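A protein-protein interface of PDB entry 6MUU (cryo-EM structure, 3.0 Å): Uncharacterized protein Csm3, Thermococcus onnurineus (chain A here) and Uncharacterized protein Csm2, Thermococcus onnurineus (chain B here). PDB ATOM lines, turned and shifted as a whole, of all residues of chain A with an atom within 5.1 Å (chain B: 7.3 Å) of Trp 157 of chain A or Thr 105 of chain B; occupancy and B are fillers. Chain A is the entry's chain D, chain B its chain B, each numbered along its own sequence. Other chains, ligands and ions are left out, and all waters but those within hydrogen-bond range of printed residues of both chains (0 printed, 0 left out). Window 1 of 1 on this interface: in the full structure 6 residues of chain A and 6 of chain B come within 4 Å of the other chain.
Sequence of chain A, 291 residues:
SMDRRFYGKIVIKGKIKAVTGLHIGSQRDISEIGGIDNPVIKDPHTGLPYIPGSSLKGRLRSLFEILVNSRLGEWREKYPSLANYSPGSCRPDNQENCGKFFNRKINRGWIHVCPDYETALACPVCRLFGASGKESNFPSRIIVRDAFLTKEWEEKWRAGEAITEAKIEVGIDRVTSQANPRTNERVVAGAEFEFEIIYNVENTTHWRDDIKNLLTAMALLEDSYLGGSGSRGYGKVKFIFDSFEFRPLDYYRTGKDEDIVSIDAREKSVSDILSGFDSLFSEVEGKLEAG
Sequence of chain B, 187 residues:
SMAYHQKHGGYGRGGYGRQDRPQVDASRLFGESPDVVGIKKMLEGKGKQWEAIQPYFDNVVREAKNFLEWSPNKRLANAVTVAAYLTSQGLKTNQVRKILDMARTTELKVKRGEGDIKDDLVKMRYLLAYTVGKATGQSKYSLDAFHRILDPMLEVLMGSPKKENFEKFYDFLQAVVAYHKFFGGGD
Among the printed residues, pairs that only touch across the chains: Thr 46 of chain A with Leu 108 of chain B, Trp 157 of chain A with Thr 105 of chain B, Trp 157 of chain A with Lys 109 of chain B and Arg 158 of chain A with Lys 109 of chain B.
OG1 of Thr 105 of chain B sits at hydrogen-bond distance from O of Asp 101 of chain B (3.2 Å).
Of the 13 printed residues of chain B, 3 touch a printed residue of chain A. Hydrophobic or aromatic side chains of chain B that line the printed part of chain A: Leu 108. Of the 12 printed residues of chain A, 3 touch a printed residue of chain B. Printed residues of chain A that touch a printed residue of chain B: Thr 46, Trp 157 and Arg 158. Hydrophobic or aromatic side chains of chain A within 4 Å of the printed part of chain B: Trp 157. Along chain A the printed residues that touch a printed residue of chain B span positions 46 to 158.
Of the printed residues of chain B, Thr 46 of chain A touches Leu 108 (3.6 Å). Of chain B, only Thr 105 (3.7 Å) and Lys 109 (3.8 Å) come within 4 Å of Trp 157 of chain A. Of the printed residues of chain B, Arg 158 of chain A touches Lys 109 (3.7 Å). Of chain A, only Trp 157 (3.7 Å) comes within 4 Å of Thr 105 of chain B. Of the printed residues of chain A, Leu 108 of chain B touches Thr 46 (3.6 Å). Of the printed residues of chain A, Lys 109 of chain B touches Trp 157 (3.8 Å) and Arg 158 (3.7 Å). The nearest printed residue of chain A that does not touch Thr 105 of chain B is Arg 158 of chain A (6.2 Å).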
ATOM      1  N   THR A  46     -21.265   5.768  15.130  1.00  0.00           N
ATOM      2  CA  THR A  46     -20.878   6.938  15.907  1.00  0.00           C
ATOM      3  C   THR A  46     -19.515   6.811  16.573  1.00  0.00           C
ATOM      4  O   THR A  46     -18.989   7.819  17.054  1.00  0.00           O
ATOM      5  CB  THR A  46     -21.919   7.240  16.990  1.00  0.00           C
ATOM      6  OG1 THR A  46     -21.898   6.200  17.969  1.00  0.00           O
ATOM      7  CG2 THR A  46     -23.308   7.321  16.384  1.00  0.00           C
ATOM      8  N   LEU A  48     -18.764   5.504  19.404  1.00  0.00           N
ATOM      9  CA  LEU A  48     -18.794   5.579  20.856  1.00  0.00           C
ATOM     10  C   LEU A  48     -18.976   4.196  21.461  1.00  0.00           C
ATOM     11  O   LEU A  48     -19.693   3.364  20.898  1.00  0.00           O
ATOM     12  CB  LEU A  48     -19.923   6.495  21.326  1.00  0.00           C
ATOM     13  CG  LEU A  48     -19.693   7.963  20.990  1.00  0.00           C
ATOM     14  CD1 LEU A  48     -20.879   8.816  21.402  1.00  0.00           C
ATOM     15  CD2 LEU A  48     -18.417   8.439  21.659  1.00  0.00           C
ATOM     16  N   TRP A 153     -23.547  12.329  27.980  1.00  0.00           N
ATOM     17  CA  TRP A 153     -22.196  11.857  27.705  1.00  0.00           C
ATOM     18  C   TRP A 153     -21.876  11.781  26.222  1.00  0.00           C
ATOM     19  O   TRP A 153     -20.723  11.508  25.872  1.00  0.00           O
ATOM     20  CB  TRP A 153     -21.978  10.500  28.367  1.00  0.00           C
ATOM     21  CG  TRP A 153     -21.828  10.634  29.825  1.00  0.00           C
ATOM     22  CD1 TRP A 153     -22.815  10.584  30.755  1.00  0.00           C
ATOM     23  CD2 TRP A 153     -20.611  10.852  30.539  1.00  0.00           C
ATOM     24  NE1 TRP A 153     -22.290  10.762  32.010  1.00  0.00           N
ATOM     25  CE2 TRP A 153     -20.935  10.924  31.903  1.00  0.00           C
ATOM     26  CE3 TRP A 153     -19.276  10.989  30.155  1.00  0.00           C
ATOM     27  CZ2 TRP A 153     -19.975  11.131  32.887  1.00  0.00           C
ATOM     28  CZ3 TRP A 153     -18.324  11.191  31.131  1.00  0.00           C
ATOM     29  CH2 TRP A 153     -18.677  11.259  32.481  1.00  0.00           C
ATOM     30  N   GLU A 154     -22.854  12.011  25.349  1.00  0.00           N
ATOM     31  CA  GLU A 154     -22.544  12.225  23.945  1.00  0.00           C
ATOM     32  C   GLU A 154     -22.049  13.644  23.705  1.00  0.00           C
ATOM     33  O   GLU A 154     -21.178  13.858  22.855  1.00  0.00           O
ATOM     34  CB  GLU A 154     -23.769  11.931  23.082  1.00  0.00           C
ATOM     35  CG  GLU A 154     -23.502  11.955  21.589  1.00  0.00           C
ATOM     36  CD  GLU A 154     -24.719  11.592  20.770  1.00  0.00           C
ATOM     37  OE1 GLU A 154     -25.795  11.378  21.366  1.00  0.00           O
ATOM     38  OE2 GLU A 154     -24.595  11.510  19.530  1.00  0.00           O
ATOM     39  N   GLU A 155     -22.564  14.614  24.469  1.00  0.00           N
ATOM     40  CA  GLU A 155     -22.084  15.989  24.368  1.00  0.00           C
ATOM     41  C   GLU A 155     -20.665  16.134  24.900  1.00  0.00           C
ATOM     42  O   GLU A 155     -19.935  17.032  24.472  1.00  0.00           O
ATOM     43  CB  GLU A 155     -23.017  16.931  25.127  1.00  0.00           C
ATOM     44  CG  GLU A 155     -24.426  16.998  24.575  1.00  0.00           C
ATOM     45  CD  GLU A 155     -24.494  17.619  23.199  1.00  0.00           C
ATOM     46  OE1 GLU A 155     -23.678  18.515  22.903  1.00  0.00           O
ATOM     47  OE2 GLU A 155     -25.371  17.213  22.411  1.00  0.00           O
ATOM     48  N   LYS A 156     -20.263  15.267  25.832  1.00  0.00           N
ATOM     49  CA  LYS A 156     -18.900  15.299  26.354  1.00  0.00           C
ATOM     50  C   LYS A 156     -17.889  14.859  25.304  1.00  0.00           C
ATOM     51  O   LYS A 156     -16.730  15.284  25.342  1.00  0.00           O
ATOM     52  CB  LYS A 156     -18.784  14.407  27.589  1.00  0.00           C
ATOM     53  CG  LYS A 156     -19.010  15.088  28.940  1.00  0.00           C
ATOM     54  CD  LYS A 156     -20.435  15.570  29.127  1.00  0.00           C
ATOM     55  CE  LYS A 156     -20.598  16.321  30.430  1.00  0.00           C
ATOM     56  NZ  LYS A 156     -20.279  15.455  31.596  1.00  0.00           N
ATOM     57  N   TRP A 157     -18.304  14.001  24.370  1.00  0.00           N
ATOM     58  CA  TRP A 157     -17.441  13.634  23.254  1.00  0.00           C
ATOM     59  C   TRP A 157     -17.348  14.760  22.235  1.00  0.00           C
ATOM     60  O   TRP A 157     -16.331  14.887  21.543  1.00  0.00           O
ATOM     61  CB  TRP A 157     -17.962  12.355  22.603  1.00  0.00           C
ATOM     62  CG  TRP A 157     -17.176  11.875  21.429  1.00  0.00           C
ATOM     63  CD1 TRP A 157     -17.529  11.969  20.123  1.00  0.00           C
ATOM     64  CD2 TRP A 157     -15.909  11.216  21.455  1.00  0.00           C
ATOM     65  NE1 TRP A 157     -16.562  11.415  19.325  1.00  0.00           N
ATOM     66  CE2 TRP A 157     -15.554  10.944  20.120  1.00  0.00           C
ATOM     67  CE3 TRP A 157     -15.036  10.834  22.474  1.00  0.00           C
ATOM     68  CZ2 TRP A 157     -14.366  10.305  19.781  1.00  0.00           C
ATOM     69  CZ3 TRP A 157     -13.858  10.198  22.137  1.00  0.00           C
ATOM     70  CH2 TRP A 157     -13.534   9.938  20.801  1.00  0.00           C
ATOM     71  N   ARG A 158     -18.395  15.581  22.131  1.00  0.00           N
ATOM     72  CA  ARG A 158     -18.357  16.744  21.252  1.00  0.00           C
ATOM     73  C   ARG A 158     -17.393  17.802  21.777  1.00  0.00           C
ATOM     74  O   ARG A 158     -16.620  18.383  21.008  1.00  0.00           O
ATOM     75  CB  ARG A 158     -19.762  17.331  21.115  1.00  0.00           C
ATOM     76  CG  ARG A 158     -20.810  16.401  20.526  1.00  0.00           C
ATOM     77  CD  ARG A 158     -20.807  16.371  19.003  1.00  0.00           C
ATOM     78  NE  ARG A 158     -19.762  15.536  18.413  1.00  0.00           N
ATOM     79  CZ  ARG A 158     -19.824  14.212  18.301  1.00  0.00           C
ATOM     80  NH1 ARG A 158     -20.880  13.545  18.743  1.00  0.00           N
ATOM     81  NH2 ARG A 158     -18.825  13.551  17.737  1.00  0.00           N
ATOM     82  N   ALA A 159     -17.421  18.059  23.083  1.00  0.00           N
ATOM     83  CA  ALA A 159     -16.616  19.105  23.695  1.00  0.00           C
ATOM     84  C   ALA A 159     -15.153  18.719  23.872  1.00  0.00           C
ATOM     85  O   ALA A 159     -14.342  19.585  24.216  1.00  0.00           O
ATOM     86  CB  ALA A 159     -17.208  19.491  25.052  1.00  0.00           C
ATOM     87  N   GLY A 160     -14.792  17.455  23.657  1.00  0.00           N
ATOM     88  CA  GLY A 160     -13.406  17.041  23.705  1.00  0.00           C
ATOM     89  C   GLY A 160     -12.984  16.292  24.950  1.00  0.00           C
ATOM     90  O   GLY A 160     -11.806  15.930  25.059  1.00  0.00           O
ATOM     91  N   GLU A 161     -13.895  16.058  25.889  1.00  0.00           N
ATOM     92  CA  GLU A 161     -13.589  15.258  27.066  1.00  0.00           C
ATOM     93  C   GLU A 161     -13.393  13.799  26.656  1.00  0.00           C
ATOM     94  O   GLU A 161     -13.972  13.325  25.676  1.00  0.00           O
ATOM     95  CB  GLU A 161     -14.719  15.405  28.092  1.00  0.00           C
ATOM     96  CG  GLU A 161     -14.491  14.769  29.461  1.00  0.00           C
ATOM     97  CD  GLU A 161     -13.406  15.459  30.269  1.00  0.00           C
ATOM     98  OE1 GLU A 161     -13.163  16.661  30.045  1.00  0.00           O
ATOM     99  OE2 GLU A 161     -12.801  14.798  31.140  1.00  0.00           O
ATOM    100  N   ILE A 163     -13.716   9.951  26.516  1.00  0.00           N
ATOM    101  CA  ILE A 163     -14.634   8.863  26.825  1.00  0.00           C
ATOM    102  C   ILE A 163     -13.881   7.577  27.131  1.00  0.00           C
ATOM    103  O   ILE A 163     -14.211   6.872  28.086  1.00  0.00           O
ATOM    104  CB  ILE A 163     -15.636   8.684  25.668  1.00  0.00           C
ATOM    105  CG1 ILE A 163     -16.522   9.919  25.567  1.00  0.00           C
ATOM    106  CG2 ILE A 163     -16.502   7.456  25.861  1.00  0.00           C
ATOM    107  CD1 ILE A 163     -17.336  10.171  26.809  1.00  0.00           C
ATOM    108  N   LEU B 100      -2.017   9.654  16.296  1.00  0.00           N
ATOM    109  CA  LEU B 100      -2.945   8.808  15.556  1.00  0.00           C
ATOM    110  C   LEU B 100      -4.357   8.891  16.127  1.00  0.00           C
ATOM    111  O   LEU B 100      -5.331   8.645  15.409  1.00  0.00           O
ATOM    112  CB  LEU B 100      -2.445   7.367  15.581  1.00  0.00           C
ATOM    113  CG  LEU B 100      -1.057   7.154  14.974  1.00  0.00           C
ATOM    114  CD1 LEU B 100      -0.569   5.735  15.186  1.00  0.00           C
ATOM    115  CD2 LEU B 100      -1.061   7.492  13.508  1.00  0.00           C
ATOM    116  N   ASP B 101      -4.477   9.235  17.412  1.00  0.00           N
ATOM    117  CA  ASP B 101      -5.783   9.438  18.029  1.00  0.00           C
ATOM    118  C   ASP B 101      -6.462  10.679  17.475  1.00  0.00           C
ATOM    119  O   ASP B 101      -7.663  10.662  17.186  1.00  0.00           O
ATOM    120  CB  ASP B 101      -5.617   9.567  19.543  1.00  0.00           C
ATOM    121  CG  ASP B 101      -6.923   9.402  20.305  1.00  0.00           C
ATOM    122  OD1 ASP B 101      -7.972   9.153  19.678  1.00  0.00           O
ATOM    123  OD2 ASP B 101      -6.893   9.524  21.549  1.00  0.00           O
ATOM    124  N   MET B 102      -5.705  11.769  17.329  1.00  0.00           N
ATOM    125  CA  MET B 102      -6.286  13.042  16.929  1.00  0.00           C
ATOM    126  C   MET B 102      -6.684  13.049  15.459  1.00  0.00           C
ATOM    127  O   MET B 102      -7.590  13.794  15.076  1.00  0.00           O
ATOM    128  CB  MET B 102      -5.296  14.167  17.242  1.00  0.00           C
ATOM    129  CG  MET B 102      -5.873  15.572  17.171  1.00  0.00           C
ATOM    130  SD  MET B 102      -7.123  15.876  18.428  1.00  0.00           S
ATOM    131  CE  MET B 102      -8.075  17.172  17.641  1.00  0.00           C
ATOM    132  N   ALA B 103      -6.048  12.220  14.633  1.00  0.00           N
ATOM    133  CA  ALA B 103      -6.490  12.080  13.251  1.00  0.00           C
ATOM    134  C   ALA B 103      -7.792  11.296  13.158  1.00  0.00           C
ATOM    135  O   ALA B 103      -8.604  11.546  12.260  1.00  0.00           O
ATOM    136  CB  ALA B 103      -5.401  11.404  12.418  1.00  0.00           C
ATOM    137  N   ARG B 104      -8.016  10.362  14.079  1.00  0.00           N
ATOM    138  CA  ARG B 104      -9.146   9.449  14.000  1.00  0.00           C
ATOM    139  C   ARG B 104     -10.406  10.015  14.644  1.00  0.00           C
ATOM    140  O   ARG B 104     -11.512   9.785  14.142  1.00  0.00           O
ATOM    141  CB  ARG B 104      -8.768   8.118  14.650  1.00  0.00           C
ATOM    142  CG  ARG B 104      -9.803   7.018  14.515  1.00  0.00           C
ATOM    143  CD  ARG B 104      -9.269   5.714  15.067  1.00  0.00           C
ATOM    144  NE  ARG B 104      -8.158   5.239  14.256  1.00  0.00           N
ATOM    145  CZ  ARG B 104      -6.899   5.186  14.668  1.00  0.00           C
ATOM    146  NH1 ARG B 104      -6.576   5.572  15.894  1.00  0.00           N
ATOM    147  NH2 ARG B 104      -5.960   4.747  13.848  1.00  0.00           N
ATOM    148  N   THR B 105     -10.264  10.744  15.754  1.00  0.00           N
ATOM    149  CA  THR B 105     -11.417  11.413  16.351  1.00  0.00           C
ATOM    150  C   THR B 105     -11.935  12.530  15.458  1.00  0.00           C
ATOM    151  O   THR B 105     -13.140  12.806  15.449  1.00  0.00           O
ATOM    152  CB  THR B 105     -11.058  11.962  17.728  1.00  0.00           C
ATOM    153  OG1 THR B 105      -9.948  12.862  17.609  1.00  0.00           O
ATOM    154  CG2 THR B 105     -10.696  10.833  18.673  1.00  0.00           C
ATOM    155  N   THR B 106     -11.047  13.177  14.702  1.00  0.00           N
ATOM    156  CA  THR B 106     -11.497  14.126  13.694  1.00  0.00           C
ATOM    157  C   THR B 106     -12.102  13.424  12.489  1.00  0.00           C
ATOM    158  O   THR B 106     -12.954  14.003  11.810  1.00  0.00           O
ATOM    159  CB  THR B 106     -10.344  15.018  13.250  1.00  0.00           C
ATOM    160  OG1 THR B 106      -9.231  14.202  12.865  1.00  0.00           O
ATOM    161  CG2 THR B 106      -9.951  15.979  14.360  1.00  0.00           C
ATOM    162  N   GLU B 107     -11.683  12.183  12.217  1.00  0.00           N
ATOM    163  CA  GLU B 107     -12.190  11.450  11.060  1.00  0.00           C
ATOM    164  C   GLU B 107     -13.670  11.124  11.205  1.00  0.00           C
ATOM    165  O   GLU B 107     -14.395  11.089  10.208  1.00  0.00           O
ATOM    166  CB  GLU B 107     -11.367  10.175  10.857  1.00  0.00           C
ATOM    167  CG  GLU B 107     -11.720   9.354   9.620  1.00  0.00           C
ATOM    168  CD  GLU B 107     -11.372  10.056   8.321  1.00  0.00           C
ATOM    169  OE1 GLU B 107     -10.455  10.901   8.320  1.00  0.00           O
ATOM    170  OE2 GLU B 107     -12.004   9.750   7.290  1.00  0.00           O
ATOM    171  N   LEU B 108     -14.146  10.924  12.433  1.00  0.00           N
ATOM    172  CA  LEU B 108     -15.582  10.824  12.649  1.00  0.00           C
ATOM    173  C   LEU B 108     -16.239  12.199  12.600  1.00  0.00           C
ATOM    174  O   LEU B 108     -17.398  12.314  12.188  1.00  0.00           O
ATOM    175  CB  LEU B 108     -15.857  10.119  13.986  1.00  0.00           C
ATOM    176  CG  LEU B 108     -17.247   9.590  14.386  1.00  0.00           C
ATOM    177  CD1 LEU B 108     -18.185  10.641  14.992  1.00  0.00           C
ATOM    178  CD2 LEU B 108     -17.911   8.914  13.196  1.00  0.00           C
ATOM    179  N   LYS B 109     -15.518  13.245  13.006  1.00  0.00           N
ATOM    180  CA  LYS B 109     -16.075  14.591  12.983  1.00  0.00           C
ATOM    181  C   LYS B 109     -16.028  15.209  11.590  1.00  0.00           C
ATOM    182  O   LYS B 109     -16.851  16.075  11.276  1.00  0.00           O
ATOM    183  CB  LYS B 109     -15.331  15.478  13.980  1.00  0.00           C
ATOM    184  CG  LYS B 109     -15.562  15.095  15.430  1.00  0.00           C
ATOM    185  CD  LYS B 109     -14.816  16.018  16.372  1.00  0.00           C
ATOM    186  CE  LYS B 109     -15.053  15.628  17.819  1.00  0.00           C
ATOM    187  NZ  LYS B 109     -14.313  16.511  18.761  1.00  0.00           N
ATOM    188  N   VAL B 110     -15.074  14.797  10.755  1.00  0.00           N
ATOM    189  CA  VAL B 110     -15.078  15.226   9.359  1.00  0.00           C
ATOM    190  C   VAL B 110     -16.173  14.505   8.586  1.00  0.00           C
ATOM    191  O   VAL B 110     -16.928  15.127   7.827  1.00  0.00           O
ATOM    192  CB  VAL B 110     -13.685  15.017   8.732  1.00  0.00           C
ATOM    193  CG1 VAL B 110     -13.733  15.144   7.218  1.00  0.00           C
ATOM    194  CG2 VAL B 110     -12.714  16.048   9.282  1.00  0.00           C
ATOM    195  N   PHE B 166      -8.533  16.440   3.862  1.00  0.00           N
ATOM    196  CA  PHE B 166      -8.235  15.635   5.042  1.00  0.00           C
ATOM    197  C   PHE B 166      -8.582  14.171   4.815  1.00  0.00           C
ATOM    198  O   PHE B 166      -7.880  13.281   5.306  1.00  0.00           O
ATOM    199  CB  PHE B 166      -8.981  16.170   6.262  1.00  0.00           C
ATOM    200  CG  PHE B 166      -8.710  15.388   7.516  1.00  0.00           C
ATOM    201  CD1 PHE B 166      -7.493  15.506   8.171  1.00  0.00           C
ATOM    202  CD2 PHE B 166      -9.667  14.529   8.037  1.00  0.00           C
ATOM    203  CE1 PHE B 166      -7.234  14.784   9.323  1.00  0.00           C
ATOM    204  CE2 PHE B 166      -9.417  13.810   9.188  1.00  0.00           C
ATOM    205  CZ  PHE B 166      -8.199  13.936   9.831  1.00  0.00           C
ATOM    206  N   TYR B 170      -5.969  11.322   5.080  1.00  0.00           N
ATOM    207  CA  TYR B 170      -6.160  10.223   6.015  1.00  0.00           C
ATOM    208  C   TYR B 170      -5.865   8.876   5.373  1.00  0.00           C
ATOM    209  O   TYR B 170      -5.513   7.923   6.075  1.00  0.00           O
ATOM    210  CB  TYR B 170      -7.587  10.262   6.553  1.00  0.00           C
ATOM    211  CG  TYR B 170      -7.851   9.321   7.692  1.00  0.00           C
ATOM    212  CD1 TYR B 170      -7.353   9.589   8.959  1.00  0.00           C
ATOM    213  CD2 TYR B 170      -8.620   8.184   7.513  1.00  0.00           C
ATOM    214  CE1 TYR B 170      -7.600   8.734  10.015  1.00  0.00           C
ATOM    215  CE2 TYR B 170      -8.878   7.331   8.560  1.00  0.00           C
ATOM    216  CZ  TYR B 170      -8.364   7.606   9.809  1.00  0.00           C
ATOM    217  OH  TYR B 170      -8.619   6.747  10.851  1.00  0.00           O
